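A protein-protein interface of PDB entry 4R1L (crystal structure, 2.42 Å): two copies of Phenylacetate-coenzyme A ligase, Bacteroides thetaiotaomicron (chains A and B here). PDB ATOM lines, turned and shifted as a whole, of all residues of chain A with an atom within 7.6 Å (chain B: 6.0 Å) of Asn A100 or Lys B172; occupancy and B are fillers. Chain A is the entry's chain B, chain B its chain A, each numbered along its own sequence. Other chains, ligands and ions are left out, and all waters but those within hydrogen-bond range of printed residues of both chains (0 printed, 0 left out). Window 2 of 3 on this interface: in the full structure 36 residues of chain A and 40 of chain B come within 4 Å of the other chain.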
ATOM      1  N   LYS A  68     -37.009 -15.177  21.442  1.00  0.00           N
ATOM      2  CA  LYS A  68     -36.058 -14.078  21.266  1.00  0.00           C
ATOM      3  C   LYS A  68     -36.712 -12.984  20.407  1.00  0.00           C
ATOM      4  O   LYS A  68     -36.429 -11.811  20.640  1.00  0.00           O
ATOM      5  CB  LYS A  68     -34.737 -14.591  20.640  1.00  0.00           C
ATOM      6  CG  LYS A  68     -33.547 -13.600  20.648  1.00  0.00           C
ATOM      7  CD  LYS A  68     -32.975 -13.328  22.054  1.00  0.00           C
ATOM      8  CE  LYS A  68     -31.702 -12.501  22.053  1.00  0.00           C
ATOM      9  NZ  LYS A  68     -30.542 -13.217  21.445  1.00  0.00           N
ATOM     10  N   MET A  71     -38.890 -10.819  22.671  1.00  0.00           N
ATOM     11  CA  MET A  71     -37.981  -9.960  23.425  1.00  0.00           C
ATOM     12  C   MET A  71     -37.469  -8.818  22.570  1.00  0.00           C
ATOM     13  O   MET A  71     -37.335  -7.702  23.071  1.00  0.00           O
ATOM     14  CB  MET A  71     -36.814 -10.756  23.981  1.00  0.00           C
ATOM     15  CG  MET A  71     -37.256 -11.711  25.098  1.00  0.00           C
ATOM     16  SD  MET A  71     -35.778 -12.452  26.077  1.00  0.00           S
ATOM     17  CE  MET A  71     -35.047 -10.848  26.823  1.00  0.00           C
ATOM     18  N   ARG A  72     -37.214  -9.072  21.281  1.00  0.00           N
ATOM     19  CA  ARG A  72     -36.805  -8.026  20.340  1.00  0.00           C
ATOM     20  C   ARG A  72     -37.948  -7.037  20.099  1.00  0.00           C
ATOM     21  O   ARG A  72     -37.713  -5.827  20.029  1.00  0.00           O
ATOM     22  CB  ARG A  72     -36.347  -8.626  19.010  1.00  0.00           C
ATOM     23  CG  ARG A  72     -35.009  -9.354  19.089  1.00  0.00           C
ATOM     24  CD  ARG A  72     -34.602  -9.809  17.710  1.00  0.00           C
ATOM     25  NE  ARG A  72     -33.322 -10.515  17.717  1.00  0.00           N
ATOM     26  CZ  ARG A  72     -33.152 -11.762  17.291  1.00  0.00           C
ATOM     27  NH1 ARG A  72     -34.177 -12.448  16.789  1.00  0.00           N
ATOM     28  NH2 ARG A  72     -31.953 -12.327  17.338  1.00  0.00           N
ATOM     29  N   TYR A  75     -38.280  -4.730  23.174  1.00  0.00           N
ATOM     30  CA  TYR A  75     -37.029  -4.084  23.536  1.00  0.00           C
ATOM     31  C   TYR A  75     -37.242  -2.574  23.757  1.00  0.00           C
ATOM     32  O   TYR A  75     -37.908  -1.921  22.954  1.00  0.00           O
ATOM     33  CB  TYR A  75     -35.953  -4.327  22.447  1.00  0.00           C
ATOM     34  CG  TYR A  75     -34.673  -3.528  22.639  1.00  0.00           C
ATOM     35  CD1 TYR A  75     -33.630  -4.014  23.431  1.00  0.00           C
ATOM     36  CD2 TYR A  75     -34.518  -2.272  22.055  1.00  0.00           C
ATOM     37  CE1 TYR A  75     -32.477  -3.249  23.663  1.00  0.00           C
ATOM     38  CE2 TYR A  75     -33.375  -1.499  22.288  1.00  0.00           C
ATOM     39  CZ  TYR A  75     -32.353  -1.996  23.082  1.00  0.00           C
ATOM     40  OH  TYR A  75     -31.227  -1.227  23.279  1.00  0.00           O
ATOM     41  N   PRO A  76     -36.641  -1.993  24.815  1.00  0.00           N
ATOM     42  CA  PRO A  76     -35.776  -2.646  25.817  1.00  0.00           C
ATOM     43  C   PRO A  76     -36.480  -3.129  27.090  1.00  0.00           C
ATOM     44  O   PRO A  76     -35.988  -4.086  27.683  1.00  0.00           O
ATOM     45  CB  PRO A  76     -34.785  -1.530  26.193  1.00  0.00           C
ATOM     46  CG  PRO A  76     -35.479  -0.217  25.851  1.00  0.00           C
ATOM     47  CD  PRO A  76     -36.725  -0.535  25.044  1.00  0.00           C
ATOM     48  N   SER A  94     -26.825  -9.268  25.755  1.00  0.00           N
ATOM     49  CA  SER A  94     -26.358 -10.502  25.108  1.00  0.00           C
ATOM     50  C   SER A  94     -25.601 -10.177  23.818  1.00  0.00           C
ATOM     51  O   SER A  94     -25.724  -9.073  23.287  1.00  0.00           O
ATOM     52  CB  SER A  94     -27.527 -11.445  24.816  1.00  0.00           C
ATOM     53  OG  SER A  94     -28.578 -10.834  24.082  1.00  0.00           O
ATOM     54  N   THR A  98     -24.986  -9.488  15.602  1.00  0.00           N
ATOM     55  CA  THR A  98     -25.876  -8.801  14.656  1.00  0.00           C
ATOM     56  C   THR A  98     -27.347  -8.832  15.142  1.00  0.00           C
ATOM     57  O   THR A  98     -27.791  -9.825  15.729  1.00  0.00           O
ATOM     58  CB  THR A  98     -25.766  -9.428  13.263  1.00  0.00           C
ATOM     59  N   GLY A  99     -28.069  -7.739  14.864  1.00  0.00           N
ATOM     60  CA  GLY A  99     -29.462  -7.512  15.250  1.00  0.00           C
ATOM     61  C   GLY A  99     -29.573  -6.417  16.300  1.00  0.00           C
ATOM     62  O   GLY A  99     -28.705  -5.535  16.365  1.00  0.00           O
ATOM     63  N   ASN A 100     -30.643  -6.453  17.129  1.00  0.00           N
ATOM     64  CA  ASN A 100     -30.793  -5.504  18.238  1.00  0.00           C
ATOM     65  C   ASN A 100     -30.607  -6.293  19.555  1.00  0.00           C
ATOM     66  O   ASN A 100     -31.485  -7.083  19.916  1.00  0.00           O
ATOM     67  CB  ASN A 100     -32.124  -4.729  18.193  1.00  0.00           C
ATOM     68  CG  ASN A 100     -32.137  -3.486  19.063  1.00  0.00           C
ATOM     69  OD1 ASN A 100     -31.336  -3.337  19.995  1.00  0.00           O
ATOM     70  ND2 ASN A 100     -33.026  -2.540  18.759  1.00  0.00           N
ATOM     71  N   PRO A 101     -29.444  -6.149  20.246  1.00  0.00           N
ATOM     72  CA  PRO A 101     -29.196  -6.955  21.464  1.00  0.00           C
ATOM     73  C   PRO A 101     -30.291  -6.822  22.526  1.00  0.00           C
ATOM     74  O   PRO A 101     -30.902  -5.768  22.685  1.00  0.00           O
ATOM     75  CB  PRO A 101     -27.873  -6.390  21.997  1.00  0.00           C
ATOM     76  CG  PRO A 101     -27.183  -5.869  20.775  1.00  0.00           C
ATOM     77  CD  PRO A 101     -28.284  -5.286  19.936  1.00  0.00           C
ATOM     78  N   THR A 102     -30.571  -7.904  23.219  1.00  0.00           N
ATOM     79  CA  THR A 102     -31.586  -7.820  24.260  1.00  0.00           C
ATOM     80  C   THR A 102     -30.903  -7.482  25.568  1.00  0.00           C
ATOM     81  O   THR A 102     -29.709  -7.774  25.764  1.00  0.00           O
ATOM     82  CB  THR A 102     -32.410  -9.083  24.363  1.00  0.00           C
ATOM     83  OG1 THR A 102     -31.508 -10.157  24.626  1.00  0.00           O
ATOM     84  CG2 THR A 102     -33.278  -9.316  23.111  1.00  0.00           C
ATOM     85  N   VAL A 103     -31.674  -6.834  26.448  1.00  0.00           N
ATOM     86  CA  VAL A 103     -31.185  -6.393  27.729  1.00  0.00           C
ATOM     87  C   VAL A 103     -31.976  -7.089  28.801  1.00  0.00           C
ATOM     88  O   VAL A 103     -33.139  -7.486  28.606  1.00  0.00           O
ATOM     89  CB  VAL A 103     -31.193  -4.835  27.904  1.00  0.00           C
ATOM     90  CG1 VAL A 103     -30.301  -4.168  26.870  1.00  0.00           C
ATOM     91  CG2 VAL A 103     -32.591  -4.234  27.884  1.00  0.00           C
ATOM     92  N   SER B 167     -18.620   4.627  20.454  1.00  0.00           N
ATOM     93  CA  SER B 167     -19.448   5.818  20.677  1.00  0.00           C
ATOM     94  C   SER B 167     -20.870   5.660  20.164  1.00  0.00           C
ATOM     95  O   SER B 167     -21.782   6.147  20.831  1.00  0.00           O
ATOM     96  CB  SER B 167     -18.834   7.044  20.029  1.00  0.00           C
ATOM     97  OG  SER B 167     -17.593   7.297  20.658  1.00  0.00           O
ATOM     98  N   LYS B 168     -21.081   4.960  19.029  1.00  0.00           N
ATOM     99  CA  LYS B 168     -22.437   4.728  18.505  1.00  0.00           C
ATOM    100  C   LYS B 168     -23.257   3.889  19.507  1.00  0.00           C
ATOM    101  O   LYS B 168     -24.433   4.165  19.702  1.00  0.00           O
ATOM    102  CB  LYS B 168     -22.413   4.063  17.121  1.00  0.00           C
ATOM    103  N   ARG B 169     -22.620   2.923  20.188  1.00  0.00           N
ATOM    104  CA  ARG B 169     -23.280   2.064  21.187  1.00  0.00           C
ATOM    105  C   ARG B 169     -23.521   2.853  22.494  1.00  0.00           C
ATOM    106  O   ARG B 169     -24.551   2.655  23.136  1.00  0.00           O
ATOM    107  CB  ARG B 169     -22.458   0.817  21.442  1.00  0.00           C
ATOM    108  CG  ARG B 169     -23.244  -0.322  22.058  1.00  0.00           C
ATOM    109  CD  ARG B 169     -22.434  -1.600  22.104  1.00  0.00           C
ATOM    110  NE  ARG B 169     -21.805  -1.893  23.396  1.00  0.00           N
ATOM    111  CZ  ARG B 169     -20.501  -2.095  23.582  1.00  0.00           C
ATOM    112  NH1 ARG B 169     -19.660  -2.071  22.551  1.00  0.00           N
ATOM    113  NH2 ARG B 169     -20.033  -2.352  24.795  1.00  0.00           N
ATOM    114  N   GLN B 170     -22.604   3.793  22.842  1.00  0.00           N
ATOM    115  CA  GLN B 170     -22.718   4.688  24.002  1.00  0.00           C
ATOM    116  C   GLN B 170     -23.954   5.578  23.871  1.00  0.00           C
ATOM    117  O   GLN B 170     -24.704   5.724  24.830  1.00  0.00           O
ATOM    118  CB  GLN B 170     -21.460   5.570  24.158  1.00  0.00           C
ATOM    119  CG  GLN B 170     -20.136   4.842  24.416  1.00  0.00           C
ATOM    120  CD  GLN B 170     -19.897   4.332  25.823  1.00  0.00           C
ATOM    121  OE1 GLN B 170     -20.610   4.646  26.776  1.00  0.00           O
ATOM    122  NE2 GLN B 170     -18.811   3.598  25.996  1.00  0.00           N
ATOM    123  N   ILE B 171     -24.170   6.147  22.665  1.00  0.00           N
ATOM    124  CA  ILE B 171     -25.295   7.017  22.295  1.00  0.00           C
ATOM    125  C   ILE B 171     -26.589   6.162  22.282  1.00  0.00           C
ATOM    126  O   ILE B 171     -27.620   6.630  22.766  1.00  0.00           O
ATOM    127  CB  ILE B 171     -24.986   7.717  20.921  1.00  0.00           C
ATOM    128  CG1 ILE B 171     -24.194   9.021  21.108  1.00  0.00           C
ATOM    129  CG2 ILE B 171     -26.237   8.068  20.108  1.00  0.00           C
ATOM    130  CD1 ILE B 171     -22.901   9.028  21.803  1.00  0.00           C
ATOM    131  N   LYS B 172     -26.517   4.911  21.787  1.00  0.00           N
ATOM    132  CA  LYS B 172     -27.663   3.984  21.772  1.00  0.00           C
ATOM    133  C   LYS B 172     -28.134   3.692  23.214  1.00  0.00           C
ATOM    134  O   LYS B 172     -29.335   3.772  23.473  1.00  0.00           O
ATOM    135  CB  LYS B 172     -27.325   2.672  21.031  1.00  0.00           C
ATOM    136  CG  LYS B 172     -28.488   1.692  21.012  1.00  0.00           C
ATOM    137  CD  LYS B 172     -28.204   0.368  20.300  1.00  0.00           C
ATOM    138  CE  LYS B 172     -29.387  -0.573  20.375  1.00  0.00           C
ATOM    139  NZ  LYS B 172     -30.635   0.041  19.835  1.00  0.00           N
ATOM    140  N   PHE B 173     -27.192   3.389  24.144  1.00  0.00           N
ATOM    141  CA  PHE B 173     -27.494   3.123  25.556  1.00  0.00           C
ATOM    142  C   PHE B 173     -28.121   4.359  26.231  1.00  0.00           C
ATOM    143  O   PHE B 173     -29.090   4.209  26.984  1.00  0.00           O
ATOM    144  CB  PHE B 173     -26.238   2.693  26.327  1.00  0.00           C
ATOM    145  CG  PHE B 173     -25.564   1.384  25.950  1.00  0.00           C
ATOM    146  CD1 PHE B 173     -26.256   0.387  25.270  1.00  0.00           C
ATOM    147  CD2 PHE B 173     -24.267   1.113  26.354  1.00  0.00           C
ATOM    148  CE1 PHE B 173     -25.641  -0.834  24.960  1.00  0.00           C
ATOM    149  CE2 PHE B 173     -23.660  -0.106  26.048  1.00  0.00           C
ATOM    150  CZ  PHE B 173     -24.350  -1.076  25.357  1.00  0.00           C
ATOM    151  N   ILE B 174     -27.595   5.573  25.931  1.00  0.00           N
ATOM    152  CA  ILE B 174     -28.104   6.835  26.492  1.00  0.00           C
ATOM    153  C   ILE B 174     -29.556   7.049  26.013  1.00  0.00           C
ATOM    154  O   ILE B 174     -30.417   7.372  26.828  1.00  0.00           O
ATOM    155  CB  ILE B 174     -27.170   8.040  26.139  1.00  0.00           C
ATOM    156  CG1 ILE B 174     -25.815   7.907  26.920  1.00  0.00           C
ATOM    157  CG2 ILE B 174     -27.848   9.414  26.439  1.00  0.00           C
ATOM    158  CD1 ILE B 174     -24.610   8.780  26.366  1.00  0.00           C
ATOM    159  N   SER B 175     -29.821   6.821  24.725  1.00  0.00           N
ATOM    160  CA  SER B 175     -31.140   7.017  24.116  1.00  0.00           C
ATOM    161  C   SER B 175     -32.162   5.962  24.578  1.00  0.00           C
ATOM    162  O   SER B 175     -33.279   6.324  24.943  1.00  0.00           O
ATOM    163  CB  SER B 175     -31.033   6.978  22.592  1.00  0.00           C
ATOM    164  OG  SER B 175     -30.134   7.977  22.129  1.00  0.00           O
ATOM    165  N   ASP B 176     -31.791   4.676  24.537  1.00  0.00           N
ATOM    166  CA  ASP B 176     -32.675   3.566  24.876  1.00  0.00           C
ATOM    167  C   ASP B 176     -32.856   3.330  26.394  1.00  0.00           C
ATOM    168  O   ASP B 176     -33.943   2.890  26.776  1.00  0.00           O
ATOM    169  CB  ASP B 176     -32.140   2.262  24.268  1.00  0.00           C
ATOM    170  CG  ASP B 176     -32.048   2.194  22.767  1.00  0.00           C
ATOM    171  OD1 ASP B 176     -32.534   3.138  22.089  1.00  0.00           O
ATOM    172  OD2 ASP B 176     -31.510   1.191  22.267  1.00  0.00           O
ATOM    173  N   PHE B 177     -31.816   3.579  27.239  1.00  0.00           N
ATOM    174  CA  PHE B 177     -31.926   3.305  28.681  1.00  0.00           C
ATOM    175  C   PHE B 177     -32.243   4.566  29.476  1.00  0.00           C
ATOM    176  O   PHE B 177     -32.462   4.483  30.690  1.00  0.00           O
ATOM    177  CB  PHE B 177     -30.625   2.652  29.238  1.00  0.00           C
ATOM    178  CG  PHE B 177     -30.154   1.432  28.468  1.00  0.00           C
ATOM    179  CD1 PHE B 177     -31.066   0.578  27.848  1.00  0.00           C
ATOM    180  CD2 PHE B 177     -28.809   1.087  28.436  1.00  0.00           C
ATOM    181  CE1 PHE B 177     -30.627  -0.537  27.133  1.00  0.00           C
ATOM    182  CE2 PHE B 177     -28.379  -0.057  27.748  1.00  0.00           C
ATOM    183  CZ  PHE B 177     -29.287  -0.840  27.082  1.00  0.00           C
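OD1 of Asn A100 lies close to NZ of Lys B172, at 3.5 Å.
OH of Tyr A75 lies within hydrogen-bond range of OD2 of Asp B176 (2.6 Å).
The side-chain amino group (NZ) of Lys B172 is in salt-bridge range of the side-chain carboxylate (OD2) of Asp B176 (2.8 Å).
Among the printed residues, pairs that only touch across the chains: Tyr A75 with Lys B172 (3.5 Å), Tyr A75 with Phe B177 (3.96 Å), Pro A76 with Asp B176 (3.6 Å) and Val A103 with Phe B177 (3.5 Å).
Asn A100 touches one residue of chain B.
Of the printed residues of chain B, Val A103 touches Phe B177.
Of chain A, only Tyr A75 and Asn A100 come within 4 Å of Lys B172.
Printed residues of chain A within 4 Å of Phe B177: Tyr A75 and Val A103.
The nearest residue of chain B that does not touch Asn A100 is Asp B176 (5.1 Å).
The nearest residue of chain A that does not touch Lys B172 is Pro A101 (4.9 Å).
Among the printed residues, 6 pairs touch across the chains.
Among the printed residues, no Asp or Glu carboxylate lies within 4 Å of a Lys or Arg side-chain nitrogen of the other chain.
No position is printed for both chains.
Of the 6 pairs that touch across the chains among the printed residues, none has its exchanged pair printed and touching as well.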
